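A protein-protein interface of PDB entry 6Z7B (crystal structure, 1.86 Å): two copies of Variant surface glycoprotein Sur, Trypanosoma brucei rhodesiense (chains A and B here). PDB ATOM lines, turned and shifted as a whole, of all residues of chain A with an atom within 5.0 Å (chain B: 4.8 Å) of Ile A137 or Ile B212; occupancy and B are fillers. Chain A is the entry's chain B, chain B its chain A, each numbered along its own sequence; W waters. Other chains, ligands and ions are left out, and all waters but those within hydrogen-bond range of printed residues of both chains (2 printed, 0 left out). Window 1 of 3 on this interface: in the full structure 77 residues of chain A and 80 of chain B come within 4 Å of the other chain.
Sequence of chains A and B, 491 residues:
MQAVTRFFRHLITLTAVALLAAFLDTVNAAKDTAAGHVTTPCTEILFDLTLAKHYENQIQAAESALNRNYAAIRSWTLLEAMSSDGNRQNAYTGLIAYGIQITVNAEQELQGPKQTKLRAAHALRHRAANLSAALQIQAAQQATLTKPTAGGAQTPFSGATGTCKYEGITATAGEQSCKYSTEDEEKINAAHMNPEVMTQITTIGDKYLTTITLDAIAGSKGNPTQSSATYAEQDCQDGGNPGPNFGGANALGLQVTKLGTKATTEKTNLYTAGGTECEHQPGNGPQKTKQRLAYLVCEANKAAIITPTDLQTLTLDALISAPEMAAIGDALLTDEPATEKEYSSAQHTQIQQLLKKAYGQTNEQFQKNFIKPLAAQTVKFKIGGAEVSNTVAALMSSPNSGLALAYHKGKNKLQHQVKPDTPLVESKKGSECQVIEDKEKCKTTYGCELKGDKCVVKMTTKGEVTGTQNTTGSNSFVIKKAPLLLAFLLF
Ile B137 touches its own counterpart, Ile A137.
Ile A137 touches Ile B212, and with the chains exchanged Ile A212 touches Ile B137.
Ile A212 touches its own counterpart, Ile B212.
4 positions are printed for both chains.
Of the 15 pairs that touch across the chains among the printed residues, 4 have their exchanged pair printed and touching as well.
Hydrophobic or aromatic side chains of chain B within 4 Å of the printed part of chain A: Ile B137, Ile B212 and Leu B214.
Among the printed residues, 15 pairs touch across the chains.
Among the printed residues, no Asp or Glu carboxylate lies within 4 Å of a Lys or Arg side-chain nitrogen of the other chain.
Of the printed residues of chain B, Ile A137 touches Ile B137, Leu B209 and Ile B212.
Of the printed residues of chain A, Ile B212 touches Ile A137 (3.99 Å), Ile A169 (3.7 Å), Thr A170 (3.0 Å), Ala A171 (2.9 Å) and Ile A212 (3.9 Å).
Printed residues of chain A within 4 Å of Leu B214: Ile A169 (2.8 Å).
Of the printed residues of chain B, Ala A171 touches Thr B210, Thr B211 and Ile B212.
Printed residues of chain B within 4 Å of Ile A212: Ile B137 (3.96 Å) and Ile B212 (3.9 Å).
Of the printed residues of chain B, Thr A170 touches Thr B211 (3.6 Å), Ile B212 (3.0 Å) and Thr B213 (3.7 Å).
Ala A139 touches none of the printed residues of chain B.
The nearest printed residue of chain A that does not touch Ile B212 is Leu A259 (4.4 Å).
Water W1 lies within hydrogen-bond range of the backbone carbonyl oxygen (O) of Thr B210 (2.6 Å) and the backbone carbonyl oxygen (O) of Gln A136 (2.7 Å).
Water W2 lies within hydrogen-bond range of the backbone carbonyl oxygen (O) of Leu B209 and the backbone carbonyl oxygen (O) of Ala A133.
Among the printed residues, pairs that only touch across the chains: Gln A136 with Leu B209 (3.8 Å), Ile A137 with Ile B137 (3.9 Å), Ile A137 with Leu B209 (3.4 Å), Ile A137 with Ile B212 (3.99 Å), Ile A169 with Ile B212 (3.7 Å), Ile A169 with Thr B213 (3.2 Å), Thr A170 with Thr B211 (3.6 Å), Thr A170 with Ile B212 (3.0 Å), Thr A170 with Thr B213 (3.7 Å), Ala A171 with Thr B210 (3.8 Å), Ala A171 with Thr B211 (3.4 Å), Ile A212 with Ile B137 (3.96 Å) and Ile A212 with Ile B212 (3.9 Å).
OG1 of Thr B210 lies within hydrogen-bond range of OG1 of Thr B211 (2.9 Å).
The side-chain amide nitrogen of Gln B138 sits at hydrogen-bond distance from the backbone carbonyl oxygen of Thr B211 (2.9 Å).
OG1 of Thr B213 lies within hydrogen-bond range of OG1 of Thr B261, 2.8 Å away.
The backbone carbonyl oxygen (O) of Thr B211 sits at hydrogen-bond distance from the side-chain hydroxyl (OG1) of Thr B261 (2.5 Å).
O of Ile B212 sits at hydrogen-bond distance from N of Ala A171 (2.9 Å).
N of Leu B214 sits at hydrogen-bond distance from O of Ile A169 (2.8 Å).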
ATOM      1  N   ALA A 133     -28.769 -22.258  -0.864  1.00  0.00           N
ATOM      2  CA  ALA A 133     -27.672 -22.475   0.066  1.00  0.00           C
ATOM      3  C   ALA A 133     -28.135 -22.302   1.510  1.00  0.00           C
ATOM      4  O   ALA A 133     -27.740 -23.075   2.388  1.00  0.00           O
ATOM      5  CB  ALA A 133     -26.518 -21.531  -0.280  1.00  0.00           C
ATOM      6  N   ALA A 134     -28.992 -21.310   1.770  1.00  0.00           N
ATOM      7  CA  ALA A 134     -29.603 -21.171   3.089  1.00  0.00           C
ATOM      8  C   ALA A 134     -30.436 -22.398   3.451  1.00  0.00           C
ATOM      9  O   ALA A 134     -30.392 -22.868   4.587  1.00  0.00           O
ATOM     10  CB  ALA A 134     -30.462 -19.904   3.136  1.00  0.00           C
ATOM     11  N   LEU A 135     -31.225 -22.912   2.510  1.00  0.00           N
ATOM     12  CA  LEU A 135     -32.042 -24.090   2.789  1.00  0.00           C
ATOM     13  C   LEU A 135     -31.181 -25.274   3.221  1.00  0.00           C
ATOM     14  O   LEU A 135     -31.578 -26.050   4.094  1.00  0.00           O
ATOM     15  CB  LEU A 135     -32.884 -24.453   1.562  1.00  0.00           C
ATOM     16  CG  LEU A 135     -33.804 -25.669   1.721  1.00  0.00           C
ATOM     17  CD1 LEU A 135     -35.257 -25.361   1.424  1.00  0.00           C
ATOM     18  CD2 LEU A 135     -33.308 -26.801   0.837  1.00  0.00           C
ATOM     19  N   GLN A 136     -30.010 -25.444   2.621  1.00  0.00           N
ATOM     20  CA  GLN A 136     -29.162 -26.561   3.029  1.00  0.00           C
ATOM     21  C   GLN A 136     -28.761 -26.424   4.494  1.00  0.00           C
ATOM     22  O   GLN A 136     -28.773 -27.405   5.243  1.00  0.00           O
ATOM     23  CB  GLN A 136     -27.934 -26.664   2.119  1.00  0.00           C
ATOM     24  CG  GLN A 136     -26.959 -27.809   2.462  1.00  0.00           C
ATOM     25  CD  GLN A 136     -27.585 -29.200   2.385  1.00  0.00           C
ATOM     26  OE1 GLN A 136     -28.230 -29.543   1.419  1.00  0.00           O
ATOM     27  NE2 GLN A 136     -27.366 -30.004   3.409  1.00  0.00           N
ATOM     28  N   ILE A 137     -28.500 -25.190   4.938  1.00  0.00           N
ATOM     29  CA  ILE A 137     -28.055 -24.945   6.300  1.00  0.00           C
ATOM     30  C   ILE A 137     -29.217 -24.987   7.271  1.00  0.00           C
ATOM     31  O   ILE A 137     -29.089 -25.529   8.374  1.00  0.00           O
ATOM     32  CB  ILE A 137     -27.296 -23.608   6.359  1.00  0.00           C
ATOM     33  CG1 ILE A 137     -25.958 -23.759   5.659  1.00  0.00           C
ATOM     34  CG2 ILE A 137     -27.046 -23.192   7.790  1.00  0.00           C
ATOM     35  CD1 ILE A 137     -25.089 -22.537   5.721  1.00  0.00           C
ATOM     36  N   GLN A 138     -30.373 -24.431   6.892  1.00  0.00           N
ATOM     37  CA  GLN A 138     -31.539 -24.440   7.773  1.00  0.00           C
ATOM     38  C   GLN A 138     -32.170 -25.819   7.897  1.00  0.00           C
ATOM     39  O   GLN A 138     -32.990 -26.027   8.797  1.00  0.00           O
ATOM     40  CB  GLN A 138     -32.583 -23.438   7.287  1.00  0.00           C
ATOM     41  CG  GLN A 138     -32.076 -22.005   7.164  1.00  0.00           C
ATOM     42  CD  GLN A 138     -31.804 -21.348   8.486  1.00  0.00           C
ATOM     43  OE1 GLN A 138     -31.908 -21.967   9.546  1.00  0.00           O
ATOM     44  NE2 GLN A 138     -31.451 -20.076   8.438  1.00  0.00           N
ATOM     45  N   ALA A 139     -31.787 -26.766   7.042  1.00  0.00           N
ATOM     46  CA  ALA A 139     -32.224 -28.146   7.179  1.00  0.00           C
ATOM     47  C   ALA A 139     -31.415 -28.932   8.192  1.00  0.00           C
ATOM     48  O   ALA A 139     -31.826 -30.033   8.553  1.00  0.00           O
ATOM     49  CB  ALA A 139     -32.149 -28.853   5.836  1.00  0.00           C
ATOM     50  N   ALA A 140     -30.285 -28.410   8.654  1.00  0.00           N
ATOM     51  CA  ALA A 140     -29.507 -29.041   9.720  1.00  0.00           C
ATOM     52  C   ALA A 140     -30.277 -28.903  11.031  1.00  0.00           C
ATOM     53  O   ALA A 140     -30.290 -27.839  11.644  1.00  0.00           O
ATOM     54  CB  ALA A 140     -28.127 -28.401   9.802  1.00  0.00           C
ATOM     55  N   ILE A 169     -19.449 -28.736  18.735  1.00  0.00           N
ATOM     56  CA  ILE A 169     -20.717 -29.372  18.395  1.00  0.00           C
ATOM     57  C   ILE A 169     -21.110 -28.928  16.988  1.00  0.00           C
ATOM     58  O   ILE A 169     -20.991 -27.748  16.646  1.00  0.00           O
ATOM     59  CB  ILE A 169     -21.793 -28.996  19.433  1.00  0.00           C
ATOM     60  CG1 ILE A 169     -21.389 -29.453  20.842  1.00  0.00           C
ATOM     61  CG2 ILE A 169     -23.160 -29.551  19.041  1.00  0.00           C
ATOM     62  CD1 ILE A 169     -22.224 -28.849  21.926  1.00  0.00           C
ATOM     63  N   THR A 170     -21.570 -29.872  16.156  1.00  0.00           N
ATOM     64  CA  THR A 170     -21.922 -29.593  14.763  1.00  0.00           C
ATOM     65  C   THR A 170     -23.313 -30.112  14.441  1.00  0.00           C
ATOM     66  O   THR A 170     -23.791 -31.084  15.030  1.00  0.00           O
ATOM     67  CB  THR A 170     -20.961 -30.233  13.755  1.00  0.00           C
ATOM     68  OG1 THR A 170     -20.944 -31.647  13.944  1.00  0.00           O
ATOM     69  CG2 THR A 170     -19.551 -29.701  13.898  1.00  0.00           C
ATOM     70  N   ALA A 171     -23.945 -29.458  13.480  1.00  0.00           N
ATOM     71  CA  ALA A 171     -25.252 -29.840  12.965  1.00  0.00           C
ATOM     72  C   ALA A 171     -25.164 -29.814  11.448  1.00  0.00           C
ATOM     73  O   ALA A 171     -24.763 -28.802  10.869  1.00  0.00           O
ATOM     74  CB  ALA A 171     -26.345 -28.898  13.471  1.00  0.00           C
ATOM     75  N   ILE A 212     -29.375 -18.413  12.641  1.00  0.00           N
ATOM     76  CA  ILE A 212     -29.446 -19.768  13.186  1.00  0.00           C
ATOM     77  C   ILE A 212     -30.329 -19.754  14.432  1.00  0.00           C
ATOM     78  O   ILE A 212     -30.244 -18.833  15.254  1.00  0.00           O
ATOM     79  CB  ILE A 212     -28.036 -20.297  13.517  1.00  0.00           C
ATOM     80  CG1 ILE A 212     -27.163 -20.375  12.268  1.00  0.00           C
ATOM     81  CG2 ILE A 212     -28.109 -21.647  14.262  1.00  0.00           C
ATOM     82  CD1 ILE A 212     -25.713 -20.089  12.584  1.00  0.00           C
ATOM     83  N   LEU A 259     -32.400 -27.575  15.797  1.00  0.00           N
ATOM     84  CA  LEU A 259     -31.932 -26.418  15.056  1.00  0.00           C
ATOM     85  C   LEU A 259     -32.825 -26.201  13.838  1.00  0.00           C
ATOM     86  O   LEU A 259     -33.571 -27.084  13.416  1.00  0.00           O
ATOM     87  CB  LEU A 259     -30.478 -26.584  14.626  1.00  0.00           C
ATOM     88  CG  LEU A 259     -29.460 -26.890  15.733  1.00  0.00           C
ATOM     89  CD1 LEU A 259     -29.189 -28.379  15.815  1.00  0.00           C
ATOM     90  CD2 LEU A 259     -28.179 -26.116  15.532  1.00  0.00           C
ATOM     91  N   ALA B 134     -23.652 -18.642   2.320  1.00  0.00           N
ATOM     92  CA  ALA B 134     -23.083 -19.388   3.450  1.00  0.00           C
ATOM     93  C   ALA B 134     -22.195 -18.483   4.306  1.00  0.00           C
ATOM     94  O   ALA B 134     -22.180 -18.586   5.536  1.00  0.00           O
ATOM     95  CB  ALA B 134     -22.303 -20.612   2.944  1.00  0.00           C
ATOM     96  N   ILE B 137     -24.206 -16.596   6.973  1.00  0.00           N
ATOM     97  CA  ILE B 137     -24.614 -17.431   8.100  1.00  0.00           C
ATOM     98  C   ILE B 137     -23.415 -17.842   8.944  1.00  0.00           C
ATOM     99  O   ILE B 137     -23.487 -17.852  10.173  1.00  0.00           O
ATOM    100  CB  ILE B 137     -25.379 -18.667   7.593  1.00  0.00           C
ATOM    101  CG1 ILE B 137     -26.812 -18.295   7.227  1.00  0.00           C
ATOM    102  CG2 ILE B 137     -25.404 -19.733   8.649  1.00  0.00           C
ATOM    103  CD1 ILE B 137     -27.527 -19.351   6.402  1.00  0.00           C
ATOM    104  N   GLN B 138     -22.309 -18.231   8.312  1.00  0.00           N
ATOM    105  CA  GLN B 138     -21.157 -18.609   9.114  1.00  0.00           C
ATOM    106  C   GLN B 138     -20.534 -17.419   9.822  1.00  0.00           C
ATOM    107  O   GLN B 138     -19.664 -17.605  10.676  1.00  0.00           O
ATOM    108  CB  GLN B 138     -20.112 -19.310   8.249  1.00  0.00           C
ATOM    109  CG  GLN B 138     -20.600 -20.567   7.528  1.00  0.00           C
ATOM    110  CD  GLN B 138     -20.899 -21.705   8.454  1.00  0.00           C
ATOM    111  OE1 GLN B 138     -20.744 -21.585   9.665  1.00  0.00           O
ATOM    112  NE2 GLN B 138     -21.322 -22.826   7.897  1.00  0.00           N
ATOM    113  N   TYR B 208     -18.267 -25.805   5.132  1.00  0.00           N
ATOM    114  CA  TYR B 208     -18.667 -24.409   5.241  1.00  0.00           C
ATOM    115  C   TYR B 208     -20.062 -24.182   4.683  1.00  0.00           C
ATOM    116  O   TYR B 208     -20.734 -23.220   5.067  1.00  0.00           O
ATOM    117  CB  TYR B 208     -17.669 -23.525   4.508  1.00  0.00           C
ATOM    118  CG  TYR B 208     -17.714 -22.047   4.867  1.00  0.00           C
ATOM    119  CD1 TYR B 208     -17.123 -21.579   6.030  1.00  0.00           C
ATOM    120  CD2 TYR B 208     -18.299 -21.111   4.022  1.00  0.00           C
ATOM    121  CE1 TYR B 208     -17.136 -20.234   6.350  1.00  0.00           C
ATOM    122  CE2 TYR B 208     -18.302 -19.759   4.339  1.00  0.00           C
ATOM    123  CZ  TYR B 208     -17.732 -19.328   5.505  1.00  0.00           C
ATOM    124  OH  TYR B 208     -17.742 -17.984   5.830  1.00  0.00           O
ATOM    125  N   LEU B 209     -20.509 -25.035   3.787  1.00  0.00           N
ATOM    126  CA  LEU B 209     -21.793 -24.837   3.163  1.00  0.00           C
ATOM    127  C   LEU B 209     -22.869 -25.738   3.758  1.00  0.00           C
ATOM    128  O   LEU B 209     -24.050 -25.517   3.511  1.00  0.00           O
ATOM    129  CB  LEU B 209     -21.644 -25.020   1.633  1.00  0.00           C
ATOM    130  CG  LEU B 209     -20.963 -23.789   0.947  1.00  0.00           C
ATOM    131  CD1 LEU B 209     -19.481 -24.002   0.555  1.00  0.00           C
ATOM    132  CD2 LEU B 209     -21.742 -23.196  -0.220  1.00  0.00           C
ATOM    133  N   THR B 210     -22.497 -26.698   4.590  1.00  0.00           N
ATOM    134  CA  THR B 210     -23.445 -27.661   5.144  1.00  0.00           C
ATOM    135  C   THR B 210     -23.583 -27.638   6.662  1.00  0.00           C
ATOM    136  O   THR B 210     -24.641 -28.024   7.165  1.00  0.00           O
ATOM    137  CB  THR B 210     -23.059 -29.096   4.725  1.00  0.00           C
ATOM    138  OG1 THR B 210     -21.854 -29.491   5.382  1.00  0.00           O
ATOM    139  CG2 THR B 210     -22.859 -29.166   3.205  1.00  0.00           C
ATOM    140  N   THR B 211     -22.571 -27.183   7.399  1.00  0.00           N
ATOM    141  CA  THR B 211     -22.425 -27.508   8.811  1.00  0.00           C
ATOM    142  C   THR B 211     -22.421 -26.259   9.681  1.00  0.00           C
ATOM    143  O   THR B 211     -21.673 -25.313   9.415  1.00  0.00           O
ATOM    144  CB  THR B 211     -21.141 -28.319   9.044  1.00  0.00           C
ATOM    145  OG1 THR B 211     -21.162 -29.500   8.239  1.00  0.00           O
ATOM    146  CG2 THR B 211     -21.044 -28.739  10.463  1.00  0.00           C
ATOM    147  N   ILE B 212     -23.252 -26.281  10.728  1.00  0.00           N
ATOM    148  CA  ILE B 212     -23.231 -25.304  11.816  1.00  0.00           C
ATOM    149  C   ILE B 212     -22.341 -25.846  12.926  1.00  0.00           C
ATOM    150  O   ILE B 212     -22.455 -27.014  13.303  1.00  0.00           O
ATOM    151  CB  ILE B 212     -24.654 -25.037  12.345  1.00  0.00           C
ATOM    152  CG1 ILE B 212     -25.514 -24.340  11.291  1.00  0.00           C
ATOM    153  CG2 ILE B 212     -24.618 -24.246  13.646  1.00  0.00           C
ATOM    154  CD1 ILE B 212     -26.971 -24.291  11.668  1.00  0.00           C
ATOM    155  N   THR B 213     -21.453 -25.007  13.449  1.00  0.00           N
ATOM    156  CA  THR B 213     -20.506 -25.414  14.477  1.00  0.00           C
ATOM    157  C   THR B 213     -20.660 -24.459  15.647  1.00  0.00           C
ATOM    158  O   THR B 213     -20.839 -23.258  15.449  1.00  0.00           O
ATOM    159  CB  THR B 213     -19.049 -25.423  13.922  1.00  0.00           C
ATOM    160  OG1 THR B 213     -18.974 -26.276  12.770  1.00  0.00           O
ATOM    161  CG2 THR B 213     -18.048 -25.921  14.947  1.00  0.00           C
ATOM    162  N   LEU B 214     -20.634 -24.995  16.866  1.00  0.00           N
ATOM    163  CA  LEU B 214     -20.856 -24.162  18.037  1.00  0.00           C
ATOM    164  C   LEU B 214     -20.098 -24.711  19.239  1.00  0.00           C
ATOM    165  O   LEU B 214     -19.780 -25.898  19.320  1.00  0.00           O
ATOM    166  CB  LEU B 214     -22.355 -24.045  18.355  1.00  0.00           C
ATOM    167  CG  LEU B 214     -23.130 -25.339  18.618  1.00  0.00           C
ATOM    168  CD1 LEU B 214     -23.203 -25.590  20.095  1.00  0.00           C
ATOM    169  CD2 LEU B 214     -24.528 -25.254  18.029  1.00  0.00           C
ATOM    170  N   THR B 261     -18.331 -22.110  11.453  1.00  0.00           N
ATOM    171  CA  THR B 261     -17.569 -23.207  10.886  1.00  0.00           C
ATOM    172  C   THR B 261     -16.334 -22.631  10.217  1.00  0.00           C
ATOM    173  O   THR B 261     -16.425 -21.626   9.506  1.00  0.00           O
ATOM    174  CB  THR B 261     -18.407 -24.001   9.875  1.00  0.00           C
ATOM    175  OG1 THR B 261     -19.525 -24.592  10.542  1.00  0.00           O
ATOM    176  CG2 THR B 261     -17.602 -25.092   9.243  1.00  0.00           C
HETATM  177  O   HOH W   1     -26.824 -29.003   6.222  1.00  0.00           O
HETATM  178  O   HOH W   2     -25.268 -24.039   1.545  1.00  0.00           O
